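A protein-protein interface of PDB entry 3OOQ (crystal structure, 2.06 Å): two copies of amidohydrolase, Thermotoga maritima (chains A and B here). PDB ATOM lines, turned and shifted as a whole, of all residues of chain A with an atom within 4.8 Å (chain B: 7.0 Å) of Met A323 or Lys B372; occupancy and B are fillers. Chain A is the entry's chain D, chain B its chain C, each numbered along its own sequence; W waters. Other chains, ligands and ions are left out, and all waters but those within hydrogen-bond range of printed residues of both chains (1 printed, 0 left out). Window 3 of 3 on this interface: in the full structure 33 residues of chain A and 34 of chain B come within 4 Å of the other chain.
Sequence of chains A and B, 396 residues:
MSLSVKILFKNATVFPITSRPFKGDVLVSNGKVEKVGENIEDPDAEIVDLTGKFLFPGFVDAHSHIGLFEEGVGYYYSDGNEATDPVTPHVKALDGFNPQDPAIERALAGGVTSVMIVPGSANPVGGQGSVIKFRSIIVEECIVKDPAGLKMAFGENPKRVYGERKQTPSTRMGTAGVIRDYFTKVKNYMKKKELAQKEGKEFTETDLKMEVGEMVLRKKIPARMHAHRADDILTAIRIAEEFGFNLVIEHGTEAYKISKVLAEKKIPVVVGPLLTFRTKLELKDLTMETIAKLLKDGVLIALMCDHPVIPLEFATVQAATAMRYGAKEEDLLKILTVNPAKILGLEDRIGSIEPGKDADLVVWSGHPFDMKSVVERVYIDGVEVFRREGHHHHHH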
ATOM      1  N   ALA A 319     -37.151  -0.055  -3.732  1.00  0.00           N
ATOM      2  CA  ALA A 319     -37.486   1.315  -4.080  1.00  0.00           C
ATOM      3  C   ALA A 319     -36.301   2.276  -3.886  1.00  0.00           C
ATOM      4  O   ALA A 319     -36.026   3.083  -4.771  1.00  0.00           O
ATOM      5  CB  ALA A 319     -38.720   1.804  -3.291  1.00  0.00           C
ATOM      6  N   ALA A 320     -35.596   2.167  -2.759  1.00  0.00           N
ATOM      7  CA  ALA A 320     -34.421   3.023  -2.509  1.00  0.00           C
ATOM      8  C   ALA A 320     -33.372   2.862  -3.605  1.00  0.00           C
ATOM      9  O   ALA A 320     -32.785   3.841  -4.054  1.00  0.00           O
ATOM     10  CB  ALA A 320     -33.797   2.733  -1.160  1.00  0.00           C
ATOM     11  N   THR A 321     -33.173   1.627  -4.052  1.00  0.00           N
ATOM     12  CA  THR A 321     -32.136   1.305  -5.033  1.00  0.00           C
ATOM     13  C   THR A 321     -32.394   1.995  -6.370  1.00  0.00           C
ATOM     14  O   THR A 321     -31.455   2.342  -7.091  1.00  0.00           O
ATOM     15  CB  THR A 321     -31.997  -0.224  -5.216  1.00  0.00           C
ATOM     16  OG1 THR A 321     -31.637  -0.805  -3.952  1.00  0.00           O
ATOM     17  CG2 THR A 321     -30.922  -0.574  -6.272  1.00  0.00           C
ATOM     18  N   ALA A 322     -33.660   2.221  -6.690  1.00  0.00           N
ATOM     19  CA  ALA A 322     -34.003   2.917  -7.933  1.00  0.00           C
ATOM     20  C   ALA A 322     -33.414   4.336  -8.037  1.00  0.00           C
ATOM     21  O   ALA A 322     -33.272   4.866  -9.145  1.00  0.00           O
ATOM     22  CB  ALA A 322     -35.515   2.923  -8.155  1.00  0.00           C
ATOM     23  N   MET A 323     -33.059   4.937  -6.900  1.00  0.00           N
ATOM     24  CA  MET A 323     -32.372   6.244  -6.891  1.00  0.00           C
ATOM     25  C   MET A 323     -31.025   6.195  -7.628  1.00  0.00           C
ATOM     26  O   MET A 323     -30.499   7.225  -8.058  1.00  0.00           O
ATOM     27  CB  MET A 323     -32.189   6.747  -5.460  1.00  0.00           C
ATOM     28  CG  MET A 323     -33.518   7.156  -4.800  1.00  0.00           C
ATOM     29  SD  MET A 323     -33.390   7.999  -3.029  1.00  0.00           S
ATOM     30  CE  MET A 323     -32.657   6.490  -2.009  1.00  0.00           C
ATOM     31  N   ARG A 324     -30.477   4.991  -7.766  1.00  0.00           N
ATOM     32  CA  ARG A 324     -29.286   4.777  -8.572  1.00  0.00           C
ATOM     33  C   ARG A 324     -29.571   4.774 -10.074  1.00  0.00           C
ATOM     34  O   ARG A 324     -28.644   4.764 -10.872  1.00  0.00           O
ATOM     35  CB  ARG A 324     -28.621   3.458  -8.188  1.00  0.00           C
ATOM     36  CG  ARG A 324     -27.947   3.516  -6.854  1.00  0.00           C
ATOM     37  CD  ARG A 324     -27.191   2.242  -6.518  1.00  0.00           C
ATOM     38  NE  ARG A 324     -26.553   2.439  -5.224  1.00  0.00           N
ATOM     39  CZ  ARG A 324     -25.772   1.560  -4.603  1.00  0.00           C
ATOM     40  NH1 ARG A 324     -25.512   0.359  -5.130  1.00  0.00           N
ATOM     41  NH2 ARG A 324     -25.256   1.903  -3.429  1.00  0.00           N
ATOM     42  N   TYR A 325     -30.849   4.796 -10.451  1.00  0.00           N
ATOM     43  CA  TYR A 325     -31.232   4.763 -11.862  1.00  0.00           C
ATOM     44  C   TYR A 325     -32.112   5.951 -12.240  1.00  0.00           C
ATOM     45  O   TYR A 325     -32.936   5.868 -13.141  1.00  0.00           O
ATOM     46  CB  TYR A 325     -31.894   3.416 -12.183  1.00  0.00           C
ATOM     47  CG  TYR A 325     -30.984   2.274 -11.801  1.00  0.00           C
ATOM     48  CD1 TYR A 325     -30.994   1.736 -10.503  1.00  0.00           C
ATOM     49  CD2 TYR A 325     -30.075   1.770 -12.718  1.00  0.00           C
ATOM     50  CE1 TYR A 325     -30.146   0.701 -10.155  1.00  0.00           C
ATOM     51  CE2 TYR A 325     -29.212   0.731 -12.385  1.00  0.00           C
ATOM     52  CZ  TYR A 325     -29.251   0.198 -11.109  1.00  0.00           C
ATOM     53  OH  TYR A 325     -28.385  -0.828 -10.786  1.00  0.00           O
ATOM     54  N   GLY A 326     -31.925   7.057 -11.535  1.00  0.00           N
ATOM     55  CA  GLY A 326     -32.546   8.317 -11.912  1.00  0.00           C
ATOM     56  C   GLY A 326     -33.945   8.537 -11.367  1.00  0.00           C
ATOM     57  O   GLY A 326     -34.587   9.520 -11.718  1.00  0.00           O
ATOM     58  N   ALA A 327     -34.435   7.625 -10.530  1.00  0.00           N
ATOM     59  CA  ALA A 327     -35.712   7.857  -9.845  1.00  0.00           C
ATOM     60  C   ALA A 327     -35.524   8.786  -8.632  1.00  0.00           C
ATOM     61  O   ALA A 327     -34.496   8.710  -7.930  1.00  0.00           O
ATOM     62  CB  ALA A 327     -36.352   6.551  -9.440  1.00  0.00           C
ATOM     63  N   GLU A 329     -36.728  10.337  -4.869  1.00  0.00           N
ATOM     64  CA  GLU A 329     -37.350   9.966  -3.592  1.00  0.00           C
ATOM     65  C   GLU A 329     -38.872  10.162  -3.554  1.00  0.00           C
ATOM     66  O   GLU A 329     -39.599   9.226  -3.221  1.00  0.00           O
ATOM     67  CB  GLU A 329     -36.702  10.757  -2.440  1.00  0.00           C
ATOM     68  CG  GLU A 329     -37.400  10.541  -1.094  1.00  0.00           C
ATOM     69  CD  GLU A 329     -36.918  11.487   0.001  1.00  0.00           C
ATOM     70  OE1 GLU A 329     -35.734  11.888  -0.026  1.00  0.00           O
ATOM     71  OE2 GLU A 329     -37.735  11.817   0.888  1.00  0.00           O
ATOM     72  N   LEU A 332     -40.701   7.807  -5.764  1.00  0.00           N
ATOM     73  CA  LEU A 332     -40.567   6.429  -5.284  1.00  0.00           C
ATOM     74  C   LEU A 332     -41.475   6.168  -4.098  1.00  0.00           C
ATOM     75  O   LEU A 332     -41.986   5.069  -3.946  1.00  0.00           O
ATOM     76  CB  LEU A 332     -39.119   6.088  -4.960  1.00  0.00           C
ATOM     77  CG  LEU A 332     -38.204   5.993  -6.181  1.00  0.00           C
ATOM     78  CD1 LEU A 332     -36.744   6.273  -5.828  1.00  0.00           C
ATOM     79  CD2 LEU A 332     -38.357   4.614  -6.814  1.00  0.00           C
ATOM     80  N   PHE A 369     -35.761   5.064   3.108  1.00  0.00           N
ATOM     81  CA  PHE A 369     -34.815   4.781   2.036  1.00  0.00           C
ATOM     82  C   PHE A 369     -33.375   4.839   2.524  1.00  0.00           C
ATOM     83  O   PHE A 369     -32.436   4.703   1.744  1.00  0.00           O
ATOM     84  CB  PHE A 369     -35.031   5.704   0.840  1.00  0.00           C
ATOM     85  CG  PHE A 369     -36.338   5.498   0.138  1.00  0.00           C
ATOM     86  CD1 PHE A 369     -37.111   4.354   0.370  1.00  0.00           C
ATOM     87  CD2 PHE A 369     -36.782   6.431  -0.803  1.00  0.00           C
ATOM     88  CE1 PHE A 369     -38.324   4.161  -0.288  1.00  0.00           C
ATOM     89  CE2 PHE A 369     -38.003   6.239  -1.474  1.00  0.00           C
ATOM     90  CZ  PHE A 369     -38.773   5.094  -1.213  1.00  0.00           C
ATOM     91  N   SER B 365     -19.647   7.728  -6.570  1.00  0.00           N
ATOM     92  CA  SER B 365     -20.086   9.120  -6.443  1.00  0.00           C
ATOM     93  C   SER B 365     -20.300   9.549  -4.984  1.00  0.00           C
ATOM     94  O   SER B 365     -20.317  10.733  -4.680  1.00  0.00           O
ATOM     95  CB  SER B 365     -21.352   9.369  -7.262  1.00  0.00           C
ATOM     96  OG  SER B 365     -22.404   8.578  -6.777  1.00  0.00           O
ATOM     97  N   GLY B 366     -20.447   8.566  -4.108  1.00  0.00           N
ATOM     98  CA  GLY B 366     -20.543   8.758  -2.670  1.00  0.00           C
ATOM     99  C   GLY B 366     -20.405   7.381  -2.064  1.00  0.00           C
ATOM    100  O   GLY B 366     -19.972   6.452  -2.745  1.00  0.00           O
ATOM    101  N   HIS B 367     -20.803   7.222  -0.808  1.00  0.00           N
ATOM    102  CA  HIS B 367     -20.631   5.951  -0.111  1.00  0.00           C
ATOM    103  C   HIS B 367     -21.445   4.827  -0.759  1.00  0.00           C
ATOM    104  O   HIS B 367     -22.628   5.000  -1.026  1.00  0.00           O
ATOM    105  CB  HIS B 367     -21.021   6.085   1.354  1.00  0.00           C
ATOM    106  CG  HIS B 367     -20.452   5.012   2.232  1.00  0.00           C
ATOM    107  ND1 HIS B 367     -20.896   3.707   2.203  1.00  0.00           N
ATOM    108  CD2 HIS B 367     -19.491   5.062   3.186  1.00  0.00           C
ATOM    109  CE1 HIS B 367     -20.213   2.989   3.078  1.00  0.00           C
ATOM    110  NE2 HIS B 367     -19.362   3.792   3.697  1.00  0.00           N
ATOM    111  N   PRO B 368     -20.820   3.662  -0.982  1.00  0.00           N
ATOM    112  CA  PRO B 368     -21.496   2.523  -1.638  1.00  0.00           C
ATOM    113  C   PRO B 368     -22.748   2.024  -0.903  1.00  0.00           C
ATOM    114  O   PRO B 368     -23.605   1.390  -1.514  1.00  0.00           O
ATOM    115  CB  PRO B 368     -20.408   1.432  -1.659  1.00  0.00           C
ATOM    116  CG  PRO B 368     -19.125   2.210  -1.710  1.00  0.00           C
ATOM    117  CD  PRO B 368     -19.376   3.421  -0.817  1.00  0.00           C
ATOM    118  N   PHE B 369     -22.863   2.322   0.390  1.00  0.00           N
ATOM    119  CA  PHE B 369     -24.046   1.916   1.133  1.00  0.00           C
ATOM    120  C   PHE B 369     -25.172   2.951   1.155  1.00  0.00           C
ATOM    121  O   PHE B 369     -26.206   2.715   1.777  1.00  0.00           O
ATOM    122  CB  PHE B 369     -23.681   1.449   2.546  1.00  0.00           C
ATOM    123  CG  PHE B 369     -22.772   0.267   2.569  1.00  0.00           C
ATOM    124  CD1 PHE B 369     -22.704  -0.606   1.480  1.00  0.00           C
ATOM    125  CD2 PHE B 369     -22.007  -0.002   3.693  1.00  0.00           C
ATOM    126  CE1 PHE B 369     -21.862  -1.702   1.508  1.00  0.00           C
ATOM    127  CE2 PHE B 369     -21.168  -1.088   3.728  1.00  0.00           C
ATOM    128  CZ  PHE B 369     -21.089  -1.948   2.634  1.00  0.00           C
ATOM    129  N   ASP B 370     -24.944   4.087   0.495  1.00  0.00           N
ATOM    130  CA  ASP B 370     -25.933   5.147   0.293  1.00  0.00           C
ATOM    131  C   ASP B 370     -26.589   4.854  -1.048  1.00  0.00           C
ATOM    132  O   ASP B 370     -25.912   4.835  -2.085  1.00  0.00           O
ATOM    133  CB  ASP B 370     -25.218   6.515   0.254  1.00  0.00           C
ATOM    134  CG  ASP B 370     -26.161   7.689  -0.018  1.00  0.00           C
ATOM    135  OD1 ASP B 370     -27.304   7.505  -0.471  1.00  0.00           O
ATOM    136  OD2 ASP B 370     -25.741   8.829   0.226  1.00  0.00           O
ATOM    137  N   MET B 371     -27.896   4.607  -1.025  1.00  0.00           N
ATOM    138  CA  MET B 371     -28.616   4.119  -2.207  1.00  0.00           C
ATOM    139  C   MET B 371     -28.671   5.145  -3.347  1.00  0.00           C
ATOM    140  O   MET B 371     -29.102   4.831  -4.463  1.00  0.00           O
ATOM    141  CB  MET B 371     -30.012   3.599  -1.817  1.00  0.00           C
ATOM    142  CG  MET B 371     -30.001   2.329  -0.940  1.00  0.00           C
ATOM    143  SD  MET B 371     -29.018   0.842  -1.811  1.00  0.00           S
ATOM    144  CE  MET B 371     -27.270   1.022  -0.944  1.00  0.00           C
ATOM    145  N   LYS B 372     -28.223   6.370  -3.058  1.00  0.00           N
ATOM    146  CA  LYS B 372     -28.021   7.395  -4.079  1.00  0.00           C
ATOM    147  C   LYS B 372     -26.683   7.284  -4.831  1.00  0.00           C
ATOM    148  O   LYS B 372     -26.552   7.840  -5.917  1.00  0.00           O
ATOM    149  CB  LYS B 372     -28.141   8.796  -3.459  1.00  0.00           C
ATOM    150  CG  LYS B 372     -29.574   9.267  -3.285  1.00  0.00           C
ATOM    151  CD  LYS B 372     -29.664  10.477  -2.371  1.00  0.00           C
ATOM    152  CE  LYS B 372     -31.128  10.892  -2.234  1.00  0.00           C
ATOM    153  NZ  LYS B 372     -31.266  11.906  -1.174  1.00  0.00           N
ATOM    154  N   SER B 373     -25.705   6.578  -4.261  1.00  0.00           N
ATOM    155  CA  SER B 373     -24.350   6.491  -4.840  1.00  0.00           C
ATOM    156  C   SER B 373     -24.266   5.626  -6.094  1.00  0.00           C
ATOM    157  O   SER B 373     -24.935   4.596  -6.197  1.00  0.00           O
ATOM    158  CB  SER B 373     -23.362   5.944  -3.814  1.00  0.00           C
ATOM    159  OG  SER B 373     -23.316   6.763  -2.673  1.00  0.00           O
ATOM    160  N   VAL B 374     -23.433   6.043  -7.044  1.00  0.00           N
ATOM    161  CA  VAL B 374     -23.197   5.247  -8.259  1.00  0.00           C
ATOM    162  C   VAL B 374     -21.710   5.048  -8.552  1.00  0.00           C
ATOM    163  O   VAL B 374     -20.875   5.863  -8.143  1.00  0.00           O
ATOM    164  CB  VAL B 374     -23.886   5.853  -9.509  1.00  0.00           C
ATOM    165  CG1 VAL B 374     -25.425   5.951  -9.292  1.00  0.00           C
ATOM    166  CG2 VAL B 374     -23.274   7.217  -9.876  1.00  0.00           C
ATOM    167  N   ARG B 388     -19.095   5.109 -16.300  1.00  0.00           N
ATOM    168  CA  ARG B 388     -20.508   5.455 -16.373  1.00  0.00           C
ATOM    169  C   ARG B 388     -20.763   6.365 -17.586  1.00  0.00           C
ATOM    170  O   ARG B 388     -20.010   7.306 -17.852  1.00  0.00           O
ATOM    171  CB  ARG B 388     -20.965   6.112 -15.071  1.00  0.00           C
ATOM    172  CG  ARG B 388     -22.450   6.446 -15.014  1.00  0.00           C
ATOM    173  CD  ARG B 388     -22.841   6.988 -13.643  1.00  0.00           C
ATOM    174  NE  ARG B 388     -24.233   7.449 -13.615  1.00  0.00           N
ATOM    175  CZ  ARG B 388     -25.285   6.674 -13.351  1.00  0.00           C
ATOM    176  NH1 ARG B 388     -25.130   5.379 -13.092  1.00  0.00           N
ATOM    177  NH2 ARG B 388     -26.509   7.199 -13.347  1.00  0.00           N
HETATM  178  O   HOH W   1     -29.705   5.194   1.260  1.00  0.00           O
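The side-chain sulfur (SD) of Met B371 is in hydrogen-bond range of the side-chain hydroxyl (OG1) of Thr A321 (3.8 Å). The backbone carbonyl oxygen (O) of Pro B368 is in hydrogen-bond range of the guanidinium group (NH2) of Arg A324 (2.6 Å). O of Ser B373 sits at hydrogen-bond distance from NE of Arg A324 (2.9 Å). The guanidinium group (NH2) of Arg A324 lies within hydrogen-bond range of the backbone carbonyl oxygen (O) of Asp B370 (3.3 Å).
The side-chain carboxylate (OD1) of Asp B370 is in hydrogen-bond range of the backbone NH (N) of Lys B372, 3.0 Å away. O of Asp B370 sits close to OG of Ser B373 (3.3 Å). N of Ser B365 sits at hydrogen-bond distance from O of Val B374, 2.7 Å away. The backbone carbonyl oxygen of Gly B366 sits close to the side-chain hydroxyl of Ser B373, at 3.4 Å. The backbone carbonyl oxygen (O) of His B367 sits at hydrogen-bond distance from the side-chain hydroxyl (OG) of Ser B373 (2.5 Å).
Ala A320 touches Met B371. Met B371 touches Met A323 (O to CB, 3.8 Å). SD of Met A323 touches CE of Lys B372, at 3.8 Å. Arg A324 touches Met B371. Val B374 touches Arg A324 (CG1 to O, 3.8 Å).
Of chain B, only Met B371 and Lys B372 come within 4 Å of Met A323. Of the printed residues of chain A, Ser B373 touches Arg A324. Of the printed residues of chain A, Met B371 touches Ala A320 (3.6 Å), Thr A321 (3.8 Å), Met A323 (3.8 Å) and Arg A324 (3.0 Å). Printed residues of chain A within 4 Å of Pro B368: Arg A324 (2.6 Å). The nearest printed residue of chain A that does not touch Met B371 is Phe A369 (4.3 Å).
Printed residues of chain B that touch a printed residue of chain A: Pro B368, Asp B370, Met B371, Lys B372, Ser B373 and Val B374. Hydrophobic or aromatic side chains of chain B within 4 Å of the printed part of chain A: Met B371 and Val B374. Along chain B the printed residues that touch a printed residue of chain A span positions 368 to 374. Of the 12 printed residues of chain A, 4 touch a printed residue of chain B. Printed residues of chain A that touch a printed residue of chain B: Ala A320, Thr A321, Met A323 and Arg A324.
Position printed for both chains: 369.
Water W1 bridges O of Phe A369 (2.8 Å) and N of Met B371 (3.0 Å).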
